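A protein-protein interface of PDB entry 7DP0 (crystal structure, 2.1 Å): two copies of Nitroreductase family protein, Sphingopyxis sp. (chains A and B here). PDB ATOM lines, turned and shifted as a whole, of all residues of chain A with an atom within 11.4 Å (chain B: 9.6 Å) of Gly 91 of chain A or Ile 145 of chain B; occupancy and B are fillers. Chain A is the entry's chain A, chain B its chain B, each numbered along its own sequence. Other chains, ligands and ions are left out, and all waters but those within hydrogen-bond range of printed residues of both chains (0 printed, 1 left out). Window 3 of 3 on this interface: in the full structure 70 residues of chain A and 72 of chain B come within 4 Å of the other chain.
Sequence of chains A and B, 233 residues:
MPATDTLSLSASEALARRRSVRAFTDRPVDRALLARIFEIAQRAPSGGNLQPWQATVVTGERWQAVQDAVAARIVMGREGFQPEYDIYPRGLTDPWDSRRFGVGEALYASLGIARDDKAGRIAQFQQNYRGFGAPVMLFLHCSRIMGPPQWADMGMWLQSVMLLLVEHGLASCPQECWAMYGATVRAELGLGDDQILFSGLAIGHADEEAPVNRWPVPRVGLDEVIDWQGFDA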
ATOM      1  N   TYR A  85       2.221 -15.264 -19.930  1.00  0.00           N
ATOM      2  CA  TYR A  85       2.467 -15.933 -18.662  1.00  0.00           C
ATOM      3  C   TYR A  85       3.471 -17.025 -18.932  1.00  0.00           C
ATOM      4  O   TYR A  85       3.839 -17.272 -20.076  1.00  0.00           O
ATOM      5  CB  TYR A  85       1.163 -16.522 -18.060  1.00  0.00           C
ATOM      6  CG  TYR A  85       0.455 -17.499 -18.995  1.00  0.00           C
ATOM      7  CD1 TYR A  85       0.774 -18.861 -18.999  1.00  0.00           C
ATOM      8  CD2 TYR A  85      -0.509 -17.054 -19.896  1.00  0.00           C
ATOM      9  CE1 TYR A  85       0.124 -19.754 -19.876  1.00  0.00           C
ATOM     10  CE2 TYR A  85      -1.137 -17.928 -20.791  1.00  0.00           C
ATOM     11  CZ  TYR A  85      -0.813 -19.271 -20.772  1.00  0.00           C
ATOM     12  OH  TYR A  85      -1.441 -20.139 -21.631  1.00  0.00           O
ATOM     13  N   ASP A  86       3.883 -17.712 -17.881  1.00  0.00           N
ATOM     14  CA  ASP A  86       4.814 -18.805 -18.048  1.00  0.00           C
ATOM     15  C   ASP A  86       4.013 -20.003 -18.529  1.00  0.00           C
ATOM     16  O   ASP A  86       3.203 -20.555 -17.782  1.00  0.00           O
ATOM     17  CB  ASP A  86       5.545 -19.093 -16.725  1.00  0.00           C
ATOM     18  CG  ASP A  86       6.642 -18.063 -16.429  1.00  0.00           C
ATOM     19  OD1 ASP A  86       7.013 -17.314 -17.357  1.00  0.00           O
ATOM     20  OD2 ASP A  86       7.110 -17.982 -15.269  1.00  0.00           O
ATOM     21  N   ILE A  87       4.213 -20.387 -19.784  1.00  0.00           N
ATOM     22  CA  ILE A  87       3.468 -21.501 -20.357  1.00  0.00           C
ATOM     23  C   ILE A  87       3.813 -22.791 -19.618  1.00  0.00           C
ATOM     24  O   ILE A  87       2.938 -23.561 -19.241  1.00  0.00           O
ATOM     25  CB  ILE A  87       3.752 -21.652 -21.862  1.00  0.00           C
ATOM     26  CG1 ILE A  87       3.184 -20.440 -22.606  1.00  0.00           C
ATOM     27  CG2 ILE A  87       3.131 -22.958 -22.426  1.00  0.00           C
ATOM     28  CD1 ILE A  87       3.300 -20.528 -24.123  1.00  0.00           C
ATOM     29  N   TYR A  88       5.102 -23.035 -19.446  1.00  0.00           N
ATOM     30  CA  TYR A  88       5.569 -24.128 -18.615  1.00  0.00           C
ATOM     31  C   TYR A  88       6.188 -23.568 -17.334  1.00  0.00           C
ATOM     32  O   TYR A  88       6.677 -22.439 -17.320  1.00  0.00           O
ATOM     33  CB  TYR A  88       6.565 -24.987 -19.397  1.00  0.00           C
ATOM     34  CG  TYR A  88       5.929 -25.677 -20.596  1.00  0.00           C
ATOM     35  CD1 TYR A  88       4.677 -26.276 -20.495  1.00  0.00           C
ATOM     36  CD2 TYR A  88       6.569 -25.698 -21.832  1.00  0.00           C
ATOM     37  CE1 TYR A  88       4.087 -26.900 -21.586  1.00  0.00           C
ATOM     38  CE2 TYR A  88       5.986 -26.313 -22.930  1.00  0.00           C
ATOM     39  CZ  TYR A  88       4.748 -26.917 -22.802  1.00  0.00           C
ATOM     40  OH  TYR A  88       4.172 -27.531 -23.889  1.00  0.00           O
ATOM     41  N   PRO A  89       6.149 -24.344 -16.243  1.00  0.00           N
ATOM     42  CA  PRO A  89       6.806 -23.890 -15.011  1.00  0.00           C
ATOM     43  C   PRO A  89       8.315 -23.710 -15.234  1.00  0.00           C
ATOM     44  O   PRO A  89       8.964 -24.567 -15.840  1.00  0.00           O
ATOM     45  CB  PRO A  89       6.518 -25.018 -14.020  1.00  0.00           C
ATOM     46  CG  PRO A  89       5.315 -25.720 -14.575  1.00  0.00           C
ATOM     47  CD  PRO A  89       5.471 -25.639 -16.065  1.00  0.00           C
ATOM     48  N   ARG A  90       8.860 -22.604 -14.744  1.00  0.00           N
ATOM     49  CA  ARG A  90      10.290 -22.327 -14.850  1.00  0.00           C
ATOM     50  C   ARG A  90      11.141 -23.424 -14.226  1.00  0.00           C
ATOM     51  O   ARG A  90      12.166 -23.821 -14.782  1.00  0.00           O
ATOM     52  CB  ARG A  90      10.597 -20.985 -14.195  1.00  0.00           C
ATOM     53  CG  ARG A  90      10.164 -19.806 -15.046  1.00  0.00           C
ATOM     54  CD  ARG A  90      10.250 -18.502 -14.282  1.00  0.00           C
ATOM     55  NE  ARG A  90       9.504 -17.453 -14.960  1.00  0.00           N
ATOM     56  CZ  ARG A  90      10.051 -16.516 -15.720  1.00  0.00           C
ATOM     57  NH1 ARG A  90       9.280 -15.607 -16.309  1.00  0.00           N
ATOM     58  NH2 ARG A  90      11.366 -16.485 -15.886  1.00  0.00           N
ATOM     59  N   GLY A  91      10.713 -23.918 -13.074  1.00  0.00           N
ATOM     60  CA  GLY A  91      11.436 -24.989 -12.418  1.00  0.00           C
ATOM     61  C   GLY A  91      10.862 -26.344 -12.794  1.00  0.00           C
ATOM     62  O   GLY A  91      10.724 -27.222 -11.934  1.00  0.00           O
ATOM     63  N   LEU A  92      10.539 -26.534 -14.073  1.00  0.00           N
ATOM     64  CA  LEU A  92       9.994 -27.819 -14.493  1.00  0.00           C
ATOM     65  C   LEU A  92      11.054 -28.904 -14.411  1.00  0.00           C
ATOM     66  O   LEU A  92      12.173 -28.744 -14.891  1.00  0.00           O
ATOM     67  CB  LEU A  92       9.439 -27.738 -15.917  1.00  0.00           C
ATOM     68  CG  LEU A  92       8.725 -28.983 -16.444  1.00  0.00           C
ATOM     69  CD1 LEU A  92       7.617 -29.365 -15.468  1.00  0.00           C
ATOM     70  CD2 LEU A  92       8.129 -28.728 -17.832  1.00  0.00           C
ATOM     71  N   THR A  93      10.659 -30.027 -13.823  1.00  0.00           N
ATOM     72  CA  THR A  93      11.524 -31.179 -13.656  1.00  0.00           C
ATOM     73  C   THR A  93      10.818 -32.441 -14.128  1.00  0.00           C
ATOM     74  O   THR A  93       9.639 -32.418 -14.472  1.00  0.00           O
ATOM     75  CB  THR A  93      11.918 -31.364 -12.181  1.00  0.00           C
ATOM     76  OG1 THR A  93      10.737 -31.652 -11.426  1.00  0.00           O
ATOM     77  CG2 THR A  93      12.540 -30.106 -11.624  1.00  0.00           C
ATOM     78  N   ASP A  94      11.528 -33.558 -14.081  1.00  0.00           N
ATOM     79  CA  ASP A  94      10.889 -34.850 -14.237  1.00  0.00           C
ATOM     80  C   ASP A  94      10.030 -35.136 -13.002  1.00  0.00           C
ATOM     81  O   ASP A  94      10.319 -34.627 -11.915  1.00  0.00           O
ATOM     82  CB  ASP A  94      11.951 -35.924 -14.463  1.00  0.00           C
ATOM     83  CG  ASP A  94      12.385 -35.985 -15.904  1.00  0.00           C
ATOM     84  OD1 ASP A  94      11.908 -35.133 -16.689  1.00  0.00           O
ATOM     85  OD2 ASP A  94      13.210 -36.855 -16.249  1.00  0.00           O
ATOM     86  N   PRO A  95       8.989 -35.976 -13.146  1.00  0.00           N
ATOM     87  CA  PRO A  95       8.590 -36.754 -14.327  1.00  0.00           C
ATOM     88  C   PRO A  95       7.997 -35.936 -15.471  1.00  0.00           C
ATOM     89  O   PRO A  95       7.908 -36.441 -16.588  1.00  0.00           O
ATOM     90  CB  PRO A  95       7.532 -37.710 -13.763  1.00  0.00           C
ATOM     91  CG  PRO A  95       6.922 -36.947 -12.637  1.00  0.00           C
ATOM     92  CD  PRO A  95       8.065 -36.195 -12.015  1.00  0.00           C
ATOM     93  N   TRP A  96       7.606 -34.698 -15.201  1.00  0.00           N
ATOM     94  CA  TRP A  96       6.815 -33.935 -16.162  1.00  0.00           C
ATOM     95  C   TRP A  96       7.521 -33.539 -17.458  1.00  0.00           C
ATOM     96  O   TRP A  96       6.956 -33.705 -18.540  1.00  0.00           O
ATOM     97  CB  TRP A  96       6.291 -32.673 -15.487  1.00  0.00           C
ATOM     98  CG  TRP A  96       5.526 -32.970 -14.248  1.00  0.00           C
ATOM     99  CD1 TRP A  96       4.258 -33.456 -14.165  1.00  0.00           C
ATOM    100  CD2 TRP A  96       6.008 -32.826 -12.902  1.00  0.00           C
ATOM    101  NE1 TRP A  96       3.904 -33.597 -12.845  1.00  0.00           N
ATOM    102  CE2 TRP A  96       4.947 -33.237 -12.060  1.00  0.00           C
ATOM    103  CE3 TRP A  96       7.198 -32.384 -12.338  1.00  0.00           C
ATOM    104  CZ2 TRP A  96       5.076 -33.208 -10.674  1.00  0.00           C
ATOM    105  CZ3 TRP A  96       7.312 -32.358 -10.972  1.00  0.00           C
ATOM    106  CH2 TRP A  96       6.253 -32.770 -10.150  1.00  0.00           C
ATOM    107  N   ASP A  97       8.753 -33.047 -17.365  1.00  0.00           N
ATOM    108  CA  ASP A  97       9.433 -32.546 -18.558  1.00  0.00           C
ATOM    109  C   ASP A  97       9.583 -33.622 -19.629  1.00  0.00           C
ATOM    110  O   ASP A  97       9.343 -33.366 -20.811  1.00  0.00           O
ATOM    111  CB  ASP A  97      10.806 -31.977 -18.204  1.00  0.00           C
ATOM    112  CG  ASP A  97      11.370 -31.104 -19.312  1.00  0.00           C
ATOM    113  OD1 ASP A  97      10.575 -30.454 -20.026  1.00  0.00           O
ATOM    114  OD2 ASP A  97      12.602 -31.078 -19.484  1.00  0.00           O
ATOM    115  N   SER A  98       9.938 -34.829 -19.204  1.00  0.00           N
ATOM    116  CA  SER A  98      10.107 -35.955 -20.120  1.00  0.00           C
ATOM    117  C   SER A  98       8.815 -36.299 -20.859  1.00  0.00           C
ATOM    118  O   SER A  98       8.867 -36.713 -22.012  1.00  0.00           O
ATOM    119  CB  SER A  98      10.608 -37.186 -19.365  1.00  0.00           C
ATOM    120  OG  SER A  98       9.663 -37.589 -18.392  1.00  0.00           O
ATOM    121  N   ARG A  99       7.664 -36.102 -20.204  1.00  0.00           N
ATOM    122  CA  ARG A  99       6.355 -36.368 -20.814  1.00  0.00           C
ATOM    123  C   ARG A  99       6.154 -35.539 -22.074  1.00  0.00           C
ATOM    124  O   ARG A  99       5.562 -36.024 -23.036  1.00  0.00           O
ATOM    125  CB  ARG A  99       5.204 -36.099 -19.829  1.00  0.00           C
ATOM    126  CG  ARG A  99       5.069 -37.144 -18.712  1.00  0.00           C
ATOM    127  CD  ARG A  99       4.218 -36.640 -17.538  1.00  0.00           C
ATOM    128  NE  ARG A  99       4.203 -37.581 -16.411  1.00  0.00           N
ATOM    129  CZ  ARG A  99       3.283 -37.597 -15.446  1.00  0.00           C
ATOM    130  NH1 ARG A  99       2.291 -36.713 -15.447  1.00  0.00           N
ATOM    131  NH2 ARG A  99       3.355 -38.495 -14.470  1.00  0.00           N
ATOM    132  N   ARG A 100       6.644 -34.297 -22.061  1.00  0.00           N
ATOM    133  CA  ARG A 100       6.562 -33.395 -23.217  1.00  0.00           C
ATOM    134  C   ARG A 100       7.222 -33.968 -24.452  1.00  0.00           C
ATOM    135  O   ARG A 100       6.676 -33.935 -25.557  1.00  0.00           O
ATOM    136  CB  ARG A 100       7.267 -32.075 -22.924  1.00  0.00           C
ATOM    137  CG  ARG A 100       6.568 -31.165 -22.003  1.00  0.00           C
ATOM    138  CD  ARG A 100       7.527 -30.152 -21.369  1.00  0.00           C
ATOM    139  NE  ARG A 100       8.467 -29.467 -22.269  1.00  0.00           N
ATOM    140  CZ  ARG A 100       8.173 -28.894 -23.438  1.00  0.00           C
ATOM    141  NH1 ARG A 100       9.134 -28.298 -24.135  1.00  0.00           N
ATOM    142  NH2 ARG A 100       6.940 -28.919 -23.932  1.00  0.00           N
ATOM    143  N   PRO A 148      -6.029 -18.906 -10.280  1.00  0.00           N
ATOM    144  CA  PRO A 148      -5.838 -20.307 -10.677  1.00  0.00           C
ATOM    145  C   PRO A 148      -7.116 -21.175 -10.698  1.00  0.00           C
ATOM    146  O   PRO A 148      -7.287 -21.934 -11.660  1.00  0.00           O
ATOM    147  CB  PRO A 148      -4.850 -20.830  -9.615  1.00  0.00           C
ATOM    148  CG  PRO A 148      -4.048 -19.610  -9.227  1.00  0.00           C
ATOM    149  CD  PRO A 148      -4.983 -18.436  -9.347  1.00  0.00           C
ATOM    150  N   LEU B  50       1.804 -32.684 -20.152  1.00  0.00           N
ATOM    151  CA  LEU B  50       2.399 -32.737 -18.821  1.00  0.00           C
ATOM    152  C   LEU B  50       1.591 -33.642 -17.884  1.00  0.00           C
ATOM    153  O   LEU B  50       2.154 -34.236 -16.962  1.00  0.00           O
ATOM    154  CB  LEU B  50       2.523 -31.335 -18.215  1.00  0.00           C
ATOM    155  CG  LEU B  50       3.542 -30.364 -18.818  1.00  0.00           C
ATOM    156  CD1 LEU B  50       3.827 -29.187 -17.866  1.00  0.00           C
ATOM    157  CD2 LEU B  50       4.797 -31.085 -19.138  1.00  0.00           C
ATOM    158  N   PRO B  52      -0.418 -32.929 -15.398  1.00  0.00           N
ATOM    159  CA  PRO B  52       0.060 -32.495 -14.081  1.00  0.00           C
ATOM    160  C   PRO B  52      -0.824 -32.935 -12.930  1.00  0.00           C
ATOM    161  O   PRO B  52      -0.367 -32.886 -11.791  1.00  0.00           O
ATOM    162  CB  PRO B  52       0.044 -30.963 -14.178  1.00  0.00           C
ATOM    163  CG  PRO B  52      -1.036 -30.658 -15.205  1.00  0.00           C
ATOM    164  CD  PRO B  52      -1.039 -31.827 -16.172  1.00  0.00           C
ATOM    165  N   GLN B  54      -2.776 -34.765 -10.034  1.00  0.00           N
ATOM    166  CA  GLN B  54      -2.577 -35.916  -9.163  1.00  0.00           C
ATOM    167  C   GLN B  54      -3.797 -36.095  -8.270  1.00  0.00           C
ATOM    168  O   GLN B  54      -4.432 -35.121  -7.880  1.00  0.00           O
ATOM    169  CB  GLN B  54      -1.310 -35.754  -8.323  1.00  0.00           C
ATOM    170  CG  GLN B  54      -0.004 -35.943  -9.073  1.00  0.00           C
ATOM    171  CD  GLN B  54       1.213 -35.617  -8.199  1.00  0.00           C
ATOM    172  OE1 GLN B  54       1.928 -34.640  -8.429  1.00  0.00           O
ATOM    173  NE2 GLN B  54       1.419 -36.424  -7.167  1.00  0.00           N
ATOM    174  N   HIS B 141      -4.876 -32.515  -6.569  1.00  0.00           N
ATOM    175  CA  HIS B 141      -3.753 -31.714  -6.116  1.00  0.00           C
ATOM    176  C   HIS B 141      -2.624 -31.826  -7.134  1.00  0.00           C
ATOM    177  O   HIS B 141      -2.630 -32.721  -7.974  1.00  0.00           O
ATOM    178  CB  HIS B 141      -3.258 -32.178  -4.729  1.00  0.00           C
ATOM    179  CG  HIS B 141      -2.951 -33.652  -4.647  1.00  0.00           C
ATOM    180  ND1 HIS B 141      -1.699 -34.159  -4.888  1.00  0.00           N
ATOM    181  CD2 HIS B 141      -3.733 -34.701  -4.309  1.00  0.00           C
ATOM    182  CE1 HIS B 141      -1.720 -35.477  -4.724  1.00  0.00           C
ATOM    183  NE2 HIS B 141      -2.949 -35.829  -4.368  1.00  0.00           N
ATOM    184  N   CYS B 142      -1.636 -30.949  -7.032  1.00  0.00           N
ATOM    185  CA  CYS B 142      -0.525 -30.983  -7.958  1.00  0.00           C
ATOM    186  C   CYS B 142       0.699 -30.376  -7.306  1.00  0.00           C
ATOM    187  O   CYS B 142       0.607 -29.747  -6.237  1.00  0.00           O
ATOM    188  CB  CYS B 142      -0.864 -30.249  -9.274  1.00  0.00           C
ATOM    189  SG  CYS B 142      -1.148 -28.441  -9.191  1.00  0.00           S
ATOM    190  N   SER B 143       1.850 -30.571  -7.940  1.00  0.00           N
ATOM    191  CA  SER B 143       3.056 -29.924  -7.462  1.00  0.00           C
ATOM    192  C   SER B 143       2.878 -28.410  -7.418  1.00  0.00           C
ATOM    193  O   SER B 143       2.170 -27.806  -8.260  1.00  0.00           O
ATOM    194  CB  SER B 143       4.256 -30.269  -8.334  1.00  0.00           C
ATOM    195  OG  SER B 143       5.336 -29.420  -8.007  1.00  0.00           O
ATOM    196  N   ARG B 144       3.543 -27.813  -6.431  1.00  0.00           N
ATOM    197  CA  ARG B 144       3.484 -26.386  -6.202  1.00  0.00           C
ATOM    198  C   ARG B 144       4.275 -25.624  -7.285  1.00  0.00           C
ATOM    199  O   ARG B 144       4.140 -24.404  -7.405  1.00  0.00           O
ATOM    200  CB  ARG B 144       4.006 -26.072  -4.786  1.00  0.00           C
ATOM    201  CG  ARG B 144       3.424 -24.805  -4.174  1.00  0.00           C
ATOM    202  CD  ARG B 144       3.739 -24.660  -2.690  1.00  0.00           C
ATOM    203  NE  ARG B 144       3.047 -25.663  -1.889  1.00  0.00           N
ATOM    204  CZ  ARG B 144       1.862 -25.481  -1.315  1.00  0.00           C
ATOM    205  NH1 ARG B 144       1.323 -26.472  -0.629  1.00  0.00           N
ATOM    206  NH2 ARG B 144       1.207 -24.323  -1.424  1.00  0.00           N
ATOM    207  N   ILE B 145       5.042 -26.345  -8.110  1.00  0.00           N
ATOM    208  CA  ILE B 145       5.748 -25.709  -9.227  1.00  0.00           C
ATOM    209  C   ILE B 145       4.815 -25.380 -10.424  1.00  0.00           C
ATOM    210  O   ILE B 145       5.148 -24.552 -11.261  1.00  0.00           O
ATOM    211  CB  ILE B 145       6.921 -26.583  -9.736  1.00  0.00           C
ATOM    212  CG1 ILE B 145       6.412 -27.708 -10.637  1.00  0.00           C
ATOM    213  CG2 ILE B 145       7.737 -27.158  -8.565  1.00  0.00           C
ATOM    214  CD1 ILE B 145       7.501 -28.426 -11.406  1.00  0.00           C
ATOM    215  N   MET B 146       3.632 -25.988 -10.470  1.00  0.00           N
ATOM    216  CA  MET B 146       2.682 -25.806 -11.593  1.00  0.00           C
ATOM    217  C   MET B 146       2.026 -24.432 -11.671  1.00  0.00           C
ATOM    218  O   MET B 146       1.704 -23.839 -10.635  1.00  0.00           O
ATOM    219  CB  MET B 146       1.578 -26.868 -11.512  1.00  0.00           C
ATOM    220  CG  MET B 146       2.132 -28.279 -11.497  1.00  0.00           C
ATOM    221  SD  MET B 146       3.021 -28.581 -13.027  1.00  0.00           S
ATOM    222  CE  MET B 146       3.799 -30.168 -12.718  1.00  0.00           C
ATOM    223  N   GLY B 147       1.818 -23.920 -12.893  1.00  0.00           N
ATOM    224  CA  GLY B 147       1.194 -22.617 -13.052  1.00  0.00           C
ATOM    225  C   GLY B 147      -0.259 -22.671 -13.498  1.00  0.00           C
ATOM    226  O   GLY B 147      -0.800 -23.747 -13.728  1.00  0.00           O
ATOM    227  N   PRO B 148      -0.898 -21.496 -13.630  1.00  0.00           N
ATOM    228  CA  PRO B 148      -2.283 -21.372 -14.119  1.00  0.00           C
ATOM    229  C   PRO B 148      -2.605 -22.243 -15.345  1.00  0.00           C
ATOM    230  O   PRO B 148      -3.662 -22.872 -15.306  1.00  0.00           O
ATOM    231  CB  PRO B 148      -2.407 -19.872 -14.473  1.00  0.00           C
ATOM    232  CG  PRO B 148      -1.480 -19.208 -13.475  1.00  0.00           C
ATOM    233  CD  PRO B 148      -0.335 -20.197 -13.212  1.00  0.00           C
ATOM    234  N   PRO B 149      -1.726 -22.309 -16.382  1.00  0.00           N
ATOM    235  CA  PRO B 149      -2.161 -23.169 -17.497  1.00  0.00           C
ATOM    236  C   PRO B 149      -2.238 -24.633 -17.062  1.00  0.00           C
ATOM    237  O   PRO B 149      -3.097 -25.369 -17.556  1.00  0.00           O
ATOM    238  CB  PRO B 149      -1.062 -22.971 -18.556  1.00  0.00           C
ATOM    239  CG  PRO B 149       0.159 -22.606 -17.742  1.00  0.00           C
ATOM    240  CD  PRO B 149      -0.376 -21.753 -16.619  1.00  0.00           C
ATOM    241  N   GLN B 150      -1.370 -25.052 -16.138  1.00  0.00           N
ATOM    242  CA  GLN B 150      -1.468 -26.421 -15.642  1.00  0.00           C
ATOM    243  C   GLN B 150      -2.692 -26.606 -14.742  1.00  0.00           C
ATOM    244  O   GLN B 150      -3.223 -27.704 -14.650  1.00  0.00           O
ATOM    245  CB  GLN B 150      -0.195 -26.843 -14.915  1.00  0.00           C
ATOM    246  CG  GLN B 150       0.953 -27.107 -15.878  1.00  0.00           C
ATOM    247  CD  GLN B 150       1.542 -25.799 -16.387  1.00  0.00           C
ATOM    248  OE1 GLN B 150       1.752 -24.866 -15.613  1.00  0.00           O
ATOM    249  NE2 GLN B 150       1.755 -25.712 -17.687  1.00  0.00           N
ATOM    250  N   TRP B 151      -3.169 -25.539 -14.111  1.00  0.00           N
ATOM    251  CA  TRP B 151      -4.422 -25.656 -13.349  1.00  0.00           C
ATOM    252  C   TRP B 151      -5.575 -25.844 -14.335  1.00  0.00           C
ATOM    253  O   TRP B 151      -6.543 -26.586 -14.077  1.00  0.00           O
ATOM    254  CB  TRP B 151      -4.625 -24.428 -12.452  1.00  0.00           C
ATOM    255  CG  TRP B 151      -3.814 -24.541 -11.189  1.00  0.00           C
ATOM    256  CD1 TRP B 151      -2.447 -24.724 -11.100  1.00  0.00           C
ATOM    257  CD2 TRP B 151      -4.303 -24.481  -9.844  1.00  0.00           C
ATOM    258  NE1 TRP B 151      -2.070 -24.787  -9.771  1.00  0.00           N
ATOM    259  CE2 TRP B 151      -3.190 -24.652  -8.983  1.00  0.00           C
ATOM    260  CE3 TRP B 151      -5.574 -24.310  -9.276  1.00  0.00           C
ATOM    261  CZ2 TRP B 151      -3.315 -24.650  -7.584  1.00  0.00           C
ATOM    262  CZ3 TRP B 151      -5.690 -24.309  -7.882  1.00  0.00           C
ATOM    263  CH2 TRP B 151      -4.569 -24.475  -7.061  1.00  0.00           C
ATOM    264  N   ASP B 193       4.513 -30.528   1.590  1.00  0.00           N
ATOM    265  CA  ASP B 193       4.215 -29.127   1.316  1.00  0.00           C
ATOM    266  C   ASP B 193       4.735 -28.750  -0.069  1.00  0.00           C
ATOM    267  O   ASP B 193       4.702 -27.584  -0.472  1.00  0.00           O
ATOM    268  CB  ASP B 193       4.814 -28.228   2.399  1.00  0.00           C
ATOM    269  CG  ASP B 193       4.017 -28.268   3.695  1.00  0.00           C
ATOM    270  OD1 ASP B 193       3.105 -29.117   3.811  1.00  0.00           O
ATOM    271  OD2 ASP B 193       4.309 -27.461   4.607  1.00  0.00           O
ATOM    272  N   ASP B 194       5.223 -29.763  -0.780  1.00  0.00           N
ATOM    273  CA  ASP B 194       5.564 -29.660  -2.194  1.00  0.00           C
ATOM    274  C   ASP B 194       4.295 -29.699  -3.033  1.00  0.00           C
ATOM    275  O   ASP B 194       4.292 -29.352  -4.218  1.00  0.00           O
ATOM    276  CB  ASP B 194       6.467 -30.810  -2.605  1.00  0.00           C
ATOM    277  CG  ASP B 194       5.712 -32.132  -2.680  1.00  0.00           C
ATOM    278  OD1 ASP B 194       5.390 -32.702  -1.611  1.00  0.00           O
ATOM    279  OD2 ASP B 194       5.422 -32.590  -3.808  1.00  0.00           O
ATOM    280  N   GLN B 195       3.218 -30.162  -2.413  1.00  0.00           N
ATOM    281  CA  GLN B 195       1.950 -30.326  -3.110  1.00  0.00           C
ATOM    282  C   GLN B 195       0.974 -29.231  -2.689  1.00  0.00           C
ATOM    283  O   GLN B 195       0.962 -28.809  -1.525  1.00  0.00           O
ATOM    284  CB  GLN B 195       1.371 -31.717  -2.820  1.00  0.00           C
ATOM    285  CG  GLN B 195       2.118 -32.881  -3.476  1.00  0.00           C
ATOM    286  CD  GLN B 195       1.871 -32.961  -4.981  1.00  0.00           C
ATOM    287  OE1 GLN B 195       0.725 -33.104  -5.430  1.00  0.00           O
ATOM    288  NE2 GLN B 195       2.937 -32.875  -5.762  1.00  0.00           N
ATOM    289  N   ILE B 196       0.139 -28.789  -3.623  1.00  0.00           N
ATOM    290  CA  ILE B 196      -0.921 -27.829  -3.310  1.00  0.00           C
ATOM    291  C   ILE B 196      -2.265 -28.476  -3.654  1.00  0.00           C
ATOM    292  O   ILE B 196      -2.421 -29.106  -4.714  1.00  0.00           O
ATOM    293  CB  ILE B 196      -0.747 -26.465  -4.073  1.00  0.00           C
ATOM    294  CG1 ILE B 196      -1.912 -25.507  -3.770  1.00  0.00           C
ATOM    295  CG2 ILE B 196      -0.591 -26.683  -5.579  1.00  0.00           C
ATOM    296  CD1 ILE B 196      -1.678 -24.048  -4.194  1.00  0.00           C
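The backbone carbonyl oxygen of Ile 87 of chain A is in hydrogen-bond range of the side-chain amide nitrogen of Gln 150 of chain B (2.9 Å). The guanidinium group of Arg 99 of chain A lies within hydrogen-bond range of the backbone carbonyl oxygen of Leu 50 of chain B (2.9 Å).
The backbone NH (N) of Ser 143 of chain B lies close to the side-chain amide nitrogen (NE2) of Gln 195 of chain B, at 3.4 Å. The side-chain carboxylate (OD2) of Asp 86 of chain A is in salt-bridge range of the guanidinium group (NE) of Arg 90 of chain A, 2.5 Å away. The side-chain amide oxygen of Gln 150 of chain B is in hydrogen-bond range of the backbone NH of Gly 147 of chain B. OG of Ser 143 of chain B lies close to N of Ile 145 of chain B, 3.1 Å away. The side-chain hydroxyl (OH) of Tyr 88 of chain A lies close to the guanidinium group (NH2) of Arg 100 of chain A (3.1 Å). NE of Arg 100 of chain A is in salt-bridge range of OD1 of Asp 97 of chain A.
Among the printed residues, pairs that only touch across the chains: Tyr 85 of chain A with Pro 149 of chain B (3.6 Å), Asp 86 of chain A with Pro 149 of chain B (3.7 Å), Ile 87 of chain A with Pro 149 of chain B (3.3 Å), Pro 89 of chain A with Ile 145 of chain B (3.1 Å), Pro 89 of chain A with Met 146 of chain B (3.98 Å), Pro 89 of chain A with Gln 150 of chain B (3.8 Å), Gly 91 of chain A with Ile 145 of chain B (3.5 Å), Trp 96 of chain A with Leu 50 of chain B (3.4 Å), Trp 96 of chain A with Ser 143 of chain B (3.7 Å), Trp 96 of chain A with Ile 145 of chain B (3.96 Å), Trp 96 of chain A with Met 146 of chain B (3.3 Å), Arg 100 of chain A with Leu 50 of chain B (3.4 Å) and Pro 148 of chain A with Trp 151 of chain B (3.6 Å).
Gly 91 of chain A touches one residue of chain B. Of chain A, only Trp 96 (3.7 Å) comes within 4 Å of Ser 143 of chain B. Of chain A, only Pro 89 (3.98 Å) and Trp 96 (3.3 Å) come within 4 Å of Met 146 of chain B. Gly 147 of chain B touches none of the printed residues of chain A. Of the printed residues of chain B, Ile 87 of chain A touches Pro 149 and Gln 150. Of the printed residues of chain B, Pro 148 of chain A touches Trp 151 (3.6 Å). Printed residues of chain B within 4 Å of Arg 100 of chain A: Leu 50 (3.4 Å). Of the printed residues of chain B, Tyr 85 of chain A touches Pro 149. Of the printed residues of chain B, Trp 96 of chain A touches Leu 50 (3.4 Å), Ser 143 (3.7 Å), Ile 145 (3.96 Å) and Met 146 (3.3 Å). Cys 142 of chain B touches none of the printed residues of chain A. The nearest residue of chain B that does not touch Gly 91 of chain A is Ser 143 of chain B (7.0 Å). The nearest printed residue of chain A that does not touch Ile 145 of chain B is Leu 92 of chain A (4.01 Å).
Printed residues of chain A that touch a printed residue of chain B: Tyr 85, Asp 86, Ile 87, Pro 89, Gly 91, Trp 96, Arg 99, Arg 100 and Pro 148. Hydrophobic or aromatic side chains of chain A that line the printed part of chain B: Tyr 85, Pro 89, Trp 96 and Pro 148. Of the 18 printed residues of chain B, 7 touch a printed residue of chain A. Along chain B the printed residues that touch a printed residue of chain A span positions 50 to 151. Among the printed residues, 15 pairs touch across the chains. Among the printed residues, no Asp or Glu carboxylate lies within 4 Å of a Lys or Arg side-chain nitrogen of the other chain.
Position printed for both chains: 148. Of the 15 pairs that touch across the chains among the printed residues, none has its exchanged pair printed and touching as well.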
